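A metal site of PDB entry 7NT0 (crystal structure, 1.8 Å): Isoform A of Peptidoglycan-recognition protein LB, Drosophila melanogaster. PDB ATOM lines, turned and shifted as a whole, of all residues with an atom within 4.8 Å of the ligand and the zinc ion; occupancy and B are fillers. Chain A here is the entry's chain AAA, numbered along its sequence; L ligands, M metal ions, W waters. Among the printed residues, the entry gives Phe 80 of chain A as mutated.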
ATOM      1  N   ALA A   6      21.793  11.039   4.715  1.00  0.00           N
ATOM      2  CA  ALA A   6      21.586   9.779   3.979  1.00  0.00           C
ATOM      3  C   ALA A   6      22.371   9.790   2.662  1.00  0.00           C
ATOM      4  O   ALA A   6      22.536   8.679   2.133  1.00  0.00           O
ATOM      5  CB  ALA A   6      20.118   9.619   3.701  1.00  0.00           C
ATOM      6  N   ASN A   7      22.721  10.990   2.131  1.00  0.00           N
ATOM      7  CA  ASN A   7      23.119  11.149   0.696  1.00  0.00           C
ATOM      8  C   ASN A   7      24.462  11.846   0.550  1.00  0.00           C
ATOM      9  O   ASN A   7      24.827  12.070  -0.589  1.00  0.00           O
ATOM     10  CB  ASN A   7      22.011  11.871  -0.087  1.00  0.00           C
ATOM     11  CG  ASN A   7      20.678  11.276   0.287  1.00  0.00           C
ATOM     12  OD1 ASN A   7      20.523  10.055   0.260  1.00  0.00           O
ATOM     13  ND2 ASN A   7      19.748  12.101   0.752  1.00  0.00           N
ATOM     14  N   GLU A  32      18.775  -4.946 -10.299  1.00  0.00           N
ATOM     15  CA  GLU A  32      17.620  -5.858 -10.218  1.00  0.00           C
ATOM     16  C   GLU A  32      16.412  -5.092 -10.724  1.00  0.00           C
ATOM     17  O   GLU A  32      16.253  -3.929 -10.316  1.00  0.00           O
ATOM     18  CB  GLU A  32      17.380  -6.311  -8.789  1.00  0.00           C
ATOM     19  CG  GLU A  32      18.576  -6.971  -8.122  1.00  0.00           C
ATOM     20  CD  GLU A  32      18.297  -7.270  -6.648  1.00  0.00           C
ATOM     21  OE1 GLU A  32      18.495  -6.349  -5.821  1.00  0.00           O
ATOM     22  OE2 GLU A  32      17.816  -8.395  -6.335  1.00  0.00           O
ATOM     23  N   HIS A  44      11.500  12.638  -2.269  1.00  0.00           N
ATOM     24  CA  HIS A  44      12.584  12.855  -1.317  1.00  0.00           C
ATOM     25  C   HIS A  44      13.141  14.252  -1.535  1.00  0.00           C
ATOM     26  O   HIS A  44      13.044  14.773  -2.660  1.00  0.00           O
ATOM     27  CB  HIS A  44      13.691  11.824  -1.561  1.00  0.00           C
ATOM     28  CG  HIS A  44      13.283  10.402  -1.429  1.00  0.00           C
ATOM     29  ND1 HIS A  44      13.422   9.678  -0.263  1.00  0.00           N
ATOM     30  CD2 HIS A  44      12.746   9.548  -2.338  1.00  0.00           C
ATOM     31  CE1 HIS A  44      13.005   8.431  -0.465  1.00  0.00           C
ATOM     32  NE2 HIS A  44      12.573   8.329  -1.736  1.00  0.00           N
ATOM     33  N   HIS A  45      13.886  14.753  -0.528  1.00  0.00           N
ATOM     34  CA  HIS A  45      14.883  15.818  -0.725  1.00  0.00           C
ATOM     35  C   HIS A  45      16.254  15.253  -0.391  1.00  0.00           C
ATOM     36  O   HIS A  45      16.315  14.216   0.256  1.00  0.00           O
ATOM     37  CB  HIS A  45      14.563  17.096   0.033  1.00  0.00           C
ATOM     38  CG  HIS A  45      14.836  17.033   1.505  1.00  0.00           C
ATOM     39  ND1 HIS A  45      14.961  18.193   2.261  1.00  0.00           N
ATOM     40  CD2 HIS A  45      14.881  16.013   2.384  1.00  0.00           C
ATOM     41  CE1 HIS A  45      15.154  17.844   3.540  1.00  0.00           C
ATOM     42  NE2 HIS A  45      15.116  16.540   3.638  1.00  0.00           N
ATOM     43  N   SER A  46      17.316  15.859  -0.869  1.00  0.00           N
ATOM     44  CA  SER A  46      18.677  15.325  -0.567  1.00  0.00           C
ATOM     45  C   SER A  46      19.093  15.734   0.836  1.00  0.00           C
ATOM     46  O   SER A  46      19.887  14.970   1.440  1.00  0.00           O
ATOM     47  CB  SER A  46      19.691  15.697  -1.621  1.00  0.00           C
ATOM     48  OG  SER A  46      19.887  17.088  -1.713  1.00  0.00           O
ATOM     49  N   HIS A  69      26.373   6.618  -1.529  1.00  0.00           N
ATOM     50  CA  HIS A  69      25.550   5.396  -1.514  1.00  0.00           C
ATOM     51  C   HIS A  69      26.397   4.151  -1.829  1.00  0.00           C
ATOM     52  O   HIS A  69      26.219   3.093  -1.154  1.00  0.00           O
ATOM     53  CB  HIS A  69      24.390   5.585  -2.476  1.00  0.00           C
ATOM     54  CG  HIS A  69      23.408   6.592  -1.984  1.00  0.00           C
ATOM     55  ND1 HIS A  69      22.288   6.920  -2.742  1.00  0.00           N
ATOM     56  CD2 HIS A  69      23.318   7.274  -0.812  1.00  0.00           C
ATOM     57  CE1 HIS A  69      21.597   7.846  -2.079  1.00  0.00           C
ATOM     58  NE2 HIS A  69      22.152   8.036  -0.858  1.00  0.00           N
ATOM     59  N   ARG A  73      27.742   3.474   1.941  1.00  0.00           N
ATOM     60  CA  ARG A  73      26.596   2.643   2.391  1.00  0.00           C
ATOM     61  C   ARG A  73      26.705   1.251   1.803  1.00  0.00           C
ATOM     62  O   ARG A  73      25.938   0.382   2.272  1.00  0.00           O
ATOM     63  CB  ARG A  73      25.271   3.354   2.095  1.00  0.00           C
ATOM     64  CG  ARG A  73      25.297   4.793   2.624  1.00  0.00           C
ATOM     65  CD  ARG A  73      23.933   5.448   2.700  1.00  0.00           C
ATOM     66  NE  ARG A  73      23.030   4.829   3.663  1.00  0.00           N
ATOM     67  CZ  ARG A  73      21.827   5.310   3.950  1.00  0.00           C
ATOM     68  NH1 ARG A  73      21.402   6.412   3.343  1.00  0.00           N
ATOM     69  NH2 ARG A  73      21.030   4.671   4.800  1.00  0.00           N
ATOM     70  N   TRP A  75      25.812   0.316  -1.237  1.00  0.00           N
ATOM     71  CA  TRP A  75      24.697  -0.015  -2.134  1.00  0.00           C
ATOM     72  C   TRP A  75      25.195  -0.236  -3.567  1.00  0.00           C
ATOM     73  O   TRP A  75      26.380   0.067  -3.903  1.00  0.00           O
ATOM     74  CB  TRP A  75      23.643   1.092  -2.058  1.00  0.00           C
ATOM     75  CG  TRP A  75      23.025   1.267  -0.715  1.00  0.00           C
ATOM     76  CD1 TRP A  75      23.091   0.479   0.407  1.00  0.00           C
ATOM     77  CD2 TRP A  75      22.199   2.387  -0.349  1.00  0.00           C
ATOM     78  NE1 TRP A  75      22.361   1.026   1.432  1.00  0.00           N
ATOM     79  CE2 TRP A  75      21.807   2.212   0.991  1.00  0.00           C
ATOM     80  CE3 TRP A  75      21.782   3.519  -1.052  1.00  0.00           C
ATOM     81  CZ2 TRP A  75      20.995   3.129   1.637  1.00  0.00           C
ATOM     82  CZ3 TRP A  75      20.943   4.396  -0.426  1.00  0.00           C
ATOM     83  CH2 TRP A  75      20.593   4.215   0.916  1.00  0.00           C
ATOM     84  N   ASN A  76      24.322  -0.769  -4.392  1.00  0.00           N
ATOM     85  CA  ASN A  76      24.581  -1.096  -5.809  1.00  0.00           C
ATOM     86  C   ASN A  76      24.797   0.187  -6.586  1.00  0.00           C
ATOM     87  O   ASN A  76      25.536   0.168  -7.572  1.00  0.00           O
ATOM     88  CB  ASN A  76      23.423  -1.900  -6.375  1.00  0.00           C
ATOM     89  CG  ASN A  76      23.453  -3.322  -5.853  1.00  0.00           C
ATOM     90  OD1 ASN A  76      22.444  -4.021  -5.814  1.00  0.00           O
ATOM     91  ND2 ASN A  76      24.636  -3.762  -5.498  1.00  0.00           N
ATOM     92  N   ASP A  77      24.144   1.264  -6.173  1.00  0.00           N
ATOM     93  CA  ASP A  77      24.060   2.455  -7.040  1.00  0.00           C
ATOM     94  C   ASP A  77      23.484   3.584  -6.177  1.00  0.00           C
ATOM     95  O   ASP A  77      23.026   3.298  -5.016  1.00  0.00           O
ATOM     96  CB  ASP A  77      23.181   2.168  -8.238  1.00  0.00           C
ATOM     97  CG  ASP A  77      23.261   3.187  -9.365  1.00  0.00           C
ATOM     98  OD1 ASP A  77      24.169   4.035  -9.326  1.00  0.00           O
ATOM     99  OD2 ASP A  77      22.389   3.122 -10.272  1.00  0.00           O
ATOM    100  N   GLY A  79      20.685   5.552  -4.669  1.00  0.00           N
ATOM    101  CA  GLY A  79      19.473   4.864  -4.186  1.00  0.00           C
ATOM    102  C   GLY A  79      18.195   5.262  -4.931  1.00  0.00           C
ATOM    103  O   GLY A  79      17.192   4.491  -4.921  1.00  0.00           O
ATOM    104  N   PHE A  80      18.192   6.472  -5.505  1.00  0.00           N
ATOM    105  CA  PHE A  80      16.985   7.089  -6.105  1.00  0.00           C
ATOM    106  C   PHE A  80      16.835   6.658  -7.564  1.00  0.00           C
ATOM    107  O   PHE A  80      17.831   6.381  -8.290  1.00  0.00           O
ATOM    108  CB  PHE A  80      17.097   8.598  -6.037  1.00  0.00           C
ATOM    109  CG  PHE A  80      17.340   9.148  -4.666  1.00  0.00           C
ATOM    110  CD1 PHE A  80      16.341   9.101  -3.727  1.00  0.00           C
ATOM    111  CD2 PHE A  80      18.535   9.741  -4.325  1.00  0.00           C
ATOM    112  CE1 PHE A  80      16.508   9.640  -2.452  1.00  0.00           C
ATOM    113  CE2 PHE A  80      18.723  10.275  -3.053  1.00  0.00           C
ATOM    114  CZ  PHE A  80      17.710  10.202  -2.104  1.00  0.00           C
ATOM    115  N   ARG A  94      18.685   5.199 -10.810  1.00  0.00           N
ATOM    116  CA  ARG A  94      18.439   3.786 -11.189  1.00  0.00           C
ATOM    117  C   ARG A  94      17.449   3.678 -12.340  1.00  0.00           C
ATOM    118  O   ARG A  94      17.519   2.680 -13.062  1.00  0.00           O
ATOM    119  CB  ARG A  94      17.915   2.987 -10.012  1.00  0.00           C
ATOM    120  CG  ARG A  94      18.914   3.010  -8.870  1.00  0.00           C
ATOM    121  CD  ARG A  94      18.661   1.906  -7.908  1.00  0.00           C
ATOM    122  NE  ARG A  94      19.633   1.973  -6.846  1.00  0.00           N
ATOM    123  CZ  ARG A  94      19.877   0.999  -5.960  1.00  0.00           C
ATOM    124  NH1 ARG A  94      19.180  -0.127  -5.976  1.00  0.00           N
ATOM    125  NH2 ARG A  94      20.812   1.146  -5.046  1.00  0.00           N
ATOM    126  N   ILE A  99      14.813  -1.835  -9.047  1.00  0.00           N
ATOM    127  CA  ILE A  99      14.623  -1.864  -7.591  1.00  0.00           C
ATOM    128  C   ILE A  99      15.550  -0.817  -6.988  1.00  0.00           C
ATOM    129  O   ILE A  99      16.749  -0.801  -7.302  1.00  0.00           O
ATOM    130  CB  ILE A  99      14.900  -3.274  -7.020  1.00  0.00           C
ATOM    131  CG1 ILE A  99      13.918  -4.306  -7.612  1.00  0.00           C
ATOM    132  CG2 ILE A  99      14.864  -3.202  -5.508  1.00  0.00           C
ATOM    133  CD1 ILE A  99      14.013  -5.711  -6.988  1.00  0.00           C
ATOM    134  N   GLY A 100      14.978   0.078  -6.205  1.00  0.00           N
ATOM    135  CA  GLY A 100      15.711   1.192  -5.609  1.00  0.00           C
ATOM    136  C   GLY A 100      16.286   0.864  -4.238  1.00  0.00           C
ATOM    137  O   GLY A 100      16.201  -0.294  -3.751  1.00  0.00           O
ATOM    138  N   ALA A 101      16.869   1.881  -3.641  1.00  0.00           N
ATOM    139  CA  ALA A 101      17.415   1.886  -2.273  1.00  0.00           C
ATOM    140  C   ALA A 101      17.095   3.251  -1.680  1.00  0.00           C
ATOM    141  O   ALA A 101      17.998   3.995  -1.351  1.00  0.00           O
ATOM    142  CB  ALA A 101      18.891   1.589  -2.293  1.00  0.00           C
ATOM    143  N   HIS A 102      15.808   3.589  -1.620  1.00  0.00           N
ATOM    144  CA  HIS A 102      15.353   4.905  -1.108  1.00  0.00           C
ATOM    145  C   HIS A 102      14.215   4.784  -0.096  1.00  0.00           C
ATOM    146  O   HIS A 102      14.101   5.714   0.699  1.00  0.00           O
ATOM    147  CB  HIS A 102      15.023   5.816  -2.311  1.00  0.00           C
ATOM    148  CG  HIS A 102      13.881   5.303  -3.104  1.00  0.00           C
ATOM    149  ND1 HIS A 102      12.607   5.697  -2.836  1.00  0.00           N
ATOM    150  CD2 HIS A 102      13.809   4.463  -4.175  1.00  0.00           C
ATOM    151  CE1 HIS A 102      11.786   5.064  -3.638  1.00  0.00           C
ATOM    152  NE2 HIS A 102      12.501   4.278  -4.466  1.00  0.00           N
ATOM    153  N   ALA A 103      13.439   3.712  -0.081  1.00  0.00           N
ATOM    154  CA  ALA A 103      12.273   3.560   0.811  1.00  0.00           C
ATOM    155  C   ALA A 103      11.964   2.081   1.025  1.00  0.00           C
ATOM    156  O   ALA A 103      11.356   1.451   0.173  1.00  0.00           O
ATOM    157  CB  ALA A 103      11.081   4.279   0.241  1.00  0.00           C
ATOM    158  N   PRO A 104      12.424   1.504   2.150  1.00  0.00           N
ATOM    159  CA  PRO A 104      12.211   0.076   2.433  1.00  0.00           C
ATOM    160  C   PRO A 104      10.729  -0.314   2.349  1.00  0.00           C
ATOM    161  O   PRO A 104       9.873   0.507   2.742  1.00  0.00           O
ATOM    162  CB  PRO A 104      12.776  -0.099   3.858  1.00  0.00           C
ATOM    163  CG  PRO A 104      13.818   0.986   3.968  1.00  0.00           C
ATOM    164  CD  PRO A 104      13.240   2.164   3.184  1.00  0.00           C
ATOM    165  N   LYS A 105      10.476  -1.475   1.746  1.00  0.00           N
ATOM    166  CA  LYS A 105       9.144  -2.075   1.477  1.00  0.00           C
ATOM    167  C   LYS A 105       8.536  -1.431   0.228  1.00  0.00           C
ATOM    168  O   LYS A 105       7.534  -1.918  -0.259  1.00  0.00           O
ATOM    169  CB  LYS A 105       8.264  -1.957   2.745  1.00  0.00           C
ATOM    170  N   ASN A 107      10.803  -0.214  -2.453  1.00  0.00           N
ATOM    171  CA  ASN A 107      11.889  -0.113  -3.433  1.00  0.00           C
ATOM    172  C   ASN A 107      11.571  -0.909  -4.690  1.00  0.00           C
ATOM    173  O   ASN A 107      12.103  -0.553  -5.774  1.00  0.00           O
ATOM    174  CB  ASN A 107      13.191  -0.568  -2.815  1.00  0.00           C
ATOM    175  CG  ASN A 107      13.772   0.468  -1.888  1.00  0.00           C
ATOM    176  OD1 ASN A 107      13.741   1.678  -2.153  1.00  0.00           O
ATOM    177  ND2 ASN A 107      14.316  -0.002  -0.788  1.00  0.00           N
ATOM    178  N   HIS A 154       8.535  10.504   1.491  1.00  0.00           N
ATOM    179  CA  HIS A 154       9.296   9.479   2.241  1.00  0.00           C
ATOM    180  C   HIS A 154       8.748   9.343   3.692  1.00  0.00           C
ATOM    181  O   HIS A 154       8.606   8.201   4.165  1.00  0.00           O
ATOM    182  CB  HIS A 154      10.784   9.812   2.193  1.00  0.00           C
ATOM    183  CG  HIS A 154      11.669   8.711   2.655  1.00  0.00           C
ATOM    184  ND1 HIS A 154      13.008   8.873   2.732  1.00  0.00           N
ATOM    185  CD2 HIS A 154      11.397   7.448   3.089  1.00  0.00           C
ATOM    186  CE1 HIS A 154      13.577   7.768   3.204  1.00  0.00           C
ATOM    187  NE2 HIS A 154      12.590   6.841   3.386  1.00  0.00           N
ATOM    188  N   ARG A 158       8.399   5.913   6.404  1.00  0.00           N
ATOM    189  CA  ARG A 158       9.640   5.701   7.189  1.00  0.00           C
ATOM    190  C   ARG A 158       9.690   6.872   8.166  1.00  0.00           C
ATOM    191  O   ARG A 158       9.180   7.964   7.847  1.00  0.00           O
ATOM    192  CB  ARG A 158      10.878   5.635   6.272  1.00  0.00           C
ATOM    193  N   CYS A 162      12.373  13.710   5.704  1.00  0.00           N
ATOM    194  CA  CYS A 162      12.385  13.698   4.211  1.00  0.00           C
ATOM    195  C   CYS A 162      10.930  13.646   3.725  1.00  0.00           C
ATOM    196  O   CYS A 162      10.179  12.776   4.175  1.00  0.00           O
ATOM    197  CB  CYS A 162      13.204  12.510   3.752  1.00  0.00           C
ATOM    198  SG  CYS A 162      13.425  12.515   1.942  1.00  0.00           S
HETATM  199  C1  LIG L   1      17.195  11.256   1.624  1.00  0.00           C
HETATM  200  C2  LIG L   1      16.815   9.830   1.555  1.00  0.00           C
HETATM  201  O1  LIG L   1      15.714   9.498   1.954  1.00  0.00           O
HETATM  202  N1  LIG L   1      17.774   9.009   1.131  1.00  0.00           N
HETATM  203  C3  LIG L   1      17.519   7.611   0.893  1.00  0.00           C
HETATM  204  C4  LIG L   1      18.444   7.077  -0.192  1.00  0.00           C
HETATM  205  C5  LIG L   1      17.647   6.741   2.147  1.00  0.00           C
HETATM  206  O2  LIG L   1      18.643   6.801   2.844  1.00  0.00           O
HETATM  207  N2  LIG L   1      16.624   5.933   2.395  1.00  0.00           N
HETATM  208  C6  LIG L   1      16.766   4.729   3.168  1.00  0.00           C
HETATM  209  C7  LIG L   1      15.759   4.668   4.347  1.00  0.00           C
HETATM  210  O3  LIG L   1      16.201   4.342   5.423  1.00  0.00           O
HETATM  211  O4  LIG L   1      14.572   5.030   4.175  1.00  0.00           O
HETATM  212  C8  LIG L   1      16.731   3.584   2.181  1.00  0.00           C
HETATM  213  C9  LIG L   1      17.397   2.358   2.698  1.00  0.00           C
HETATM  214  C10 LIG L   1      17.132   1.259   1.717  1.00  0.00           C
HETATM  215  O5  LIG L   1      16.091   1.183   1.064  1.00  0.00           O
HETATM  216  N3  LIG L   1      18.125   0.374   1.631  1.00  0.00           N
HETATM  217  C11 LIG L   1      17.964  -0.825   0.851  1.00  0.00           C
HETATM  218  C12 LIG L   1      16.917  -1.765   1.482  1.00  0.00           C
HETATM  219  O6  LIG L   1      16.748  -1.728   2.696  1.00  0.00           O
HETATM  220  N4  LIG L   1      16.152  -2.531   0.686  1.00  0.00           N
HETATM  221  C13 LIG L   1      15.130  -3.470   1.194  1.00  0.00           C
HETATM  222  C14 LIG L   1      15.345  -4.862   0.599  1.00  0.00           C
HETATM  223  C15 LIG L   1      13.655  -3.097   0.867  1.00  0.00           C
HETATM  224  O7  LIG L   1      13.390  -2.672  -0.262  1.00  0.00           O
HETATM  225  O8  LIG L   1      12.805  -3.331   1.738  1.00  0.00           O
HETATM  226  C16 LIG L   1      19.382  -1.376   0.709  1.00  0.00           C
HETATM  227  C17 LIG L   1      19.577  -1.994  -0.635  1.00  0.00           C
HETATM  228  C18 LIG L   1      20.994  -2.414  -0.967  1.00  0.00           C
HETATM  229  C19 LIG L   1      21.096  -3.046  -2.352  1.00  0.00           C
HETATM  230  C20 LIG L   1      20.802  -1.997  -3.445  1.00  0.00           C
HETATM  231  O9  LIG L   1      21.584  -1.034  -3.563  1.00  0.00           O
HETATM  232  O10 LIG L   1      19.841  -2.230  -4.178  1.00  0.00           O
HETATM  233  N5  LIG L   1      20.122  -4.161  -2.450  1.00  0.00           N
HETATM  234 ZN    ZN M   1      14.002  10.373   1.614  1.00  0.00          ZN
HETATM  235  O   HOH W   1      18.815   5.809   6.022  1.00  0.00           O
HETATM  236  O   HOH W   2      16.465  -2.472  -2.138  1.00  0.00           O
HETATM  237  O   HOH W   3      16.218   9.955   5.116  1.00  0.00           O
HETATM  238  O   HOH W   4      11.058  -2.986  -1.419  1.00  0.00           O
HETATM  239  O   HOH W   5      20.195   0.335   3.663  1.00  0.00           O
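The backbone NH (N) of Lys 105 is in hydrogen-bond range of an oxygen (O8) of the ligand. O of His 102 is in hydrogen-bond range of N2 of the ligand. N1 of the ligand is in hydrogen-bond range of OD1 of Asn 7. The guanidinium group of Arg 73 sits at hydrogen-bond distance from an oxygen (O2) of the ligand (2.8 Å). ND2 of Asn 107 lies within hydrogen-bond range of O5 of the ligand (2.8 Å). The backbone NH (N) of Asn 76 lies within hydrogen-bond range of an oxygen (O9) of the ligand (2.9 Å). O9 of the ligand is in salt-bridge range of NH2 of Arg 94 (2.7 Å).
A ring nitrogen (ND1) of His 69 is in hydrogen-bond range of the backbone NH (N) of Gly 79. The backbone carbonyl oxygen of Asn 107 lies within hydrogen-bond range of the backbone NH of Gly 100. OD1 of Asn 107 lies within hydrogen-bond range of N of His 102 (2.9 Å). The side-chain amide oxygen of Asn 107 lies within hydrogen-bond range of the backbone NH of Ala 103 (2.9 Å). The guanidinium group (NH1) of Arg 73 is in hydrogen-bond range of the backbone carbonyl oxygen (O) of Ala 6, at 2.8 Å. N of Ala 101 lies within hydrogen-bond range of OD1 of Asn 107 (3.5 Å). NE2 of His 69 is in hydrogen-bond range of OD1 of Asn 7. The backbone carbonyl oxygen of Ser 46 is in hydrogen-bond range of the side-chain amide nitrogen of Asn 7 (3.0 Å).
Ala 6 touches the ligand. His 45 touches the ligand (O to C1, 3.4 Å). His 69 touches the ligand (CE1 to C4, 3.8 Å). Trp 75 touches the ligand (CB to O9, 3.3 Å). CZ of Phe 80 touches N1 of the ligand (3.4 Å). Ala 101 touches the ligand (O to C4, 3.3 Å). Ala 103 touches the ligand. CD of Pro 104 touches O4 of the ligand (3.3 Å). Hydrophobic or aromatic side chains that line the ligand: Ala 6, His 44, His 69, Trp 75, Phe 80, Ala 101, Pro 104 and His 154. The nearest printed residue that does not touch the ligand is Gly 100 (4.1 Å).
Three residues have an atom within 4 Å of the zinc ion: His 44, His 154 and Cys 162. The nearest printed residue that does not touch the zinc ion is His 45 (4.7 Å).
The zinc ion is bound by an oxygen (O1) of the ligand (2.0 Å), a ring nitrogen (ND1) of His 44 (2.1 Å), a ring nitrogen (ND1) of His 154 (2.1 Å) and the side-chain sulfur of Cys 162 (2.2 Å). The zinc ion has four donor atoms within binding distance.
Water W4 bridges O7 of the ligand and N of Asn 107. Water W2 lies within hydrogen-bond range of the backbone carbonyl oxygen of Gly 100 (2.7 Å) and a nitrogen (N4) of the ligand (2.8 Å). Water W5 lies within hydrogen-bond range of N3 of the ligand (2.9 Å) and NE1 of Trp 75 (3.2 Å). Water W1 lies within hydrogen-bond range of the guanidinium group of Arg 73 (2.8 Å) and an oxygen (O3) of the ligand (3.1 Å).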
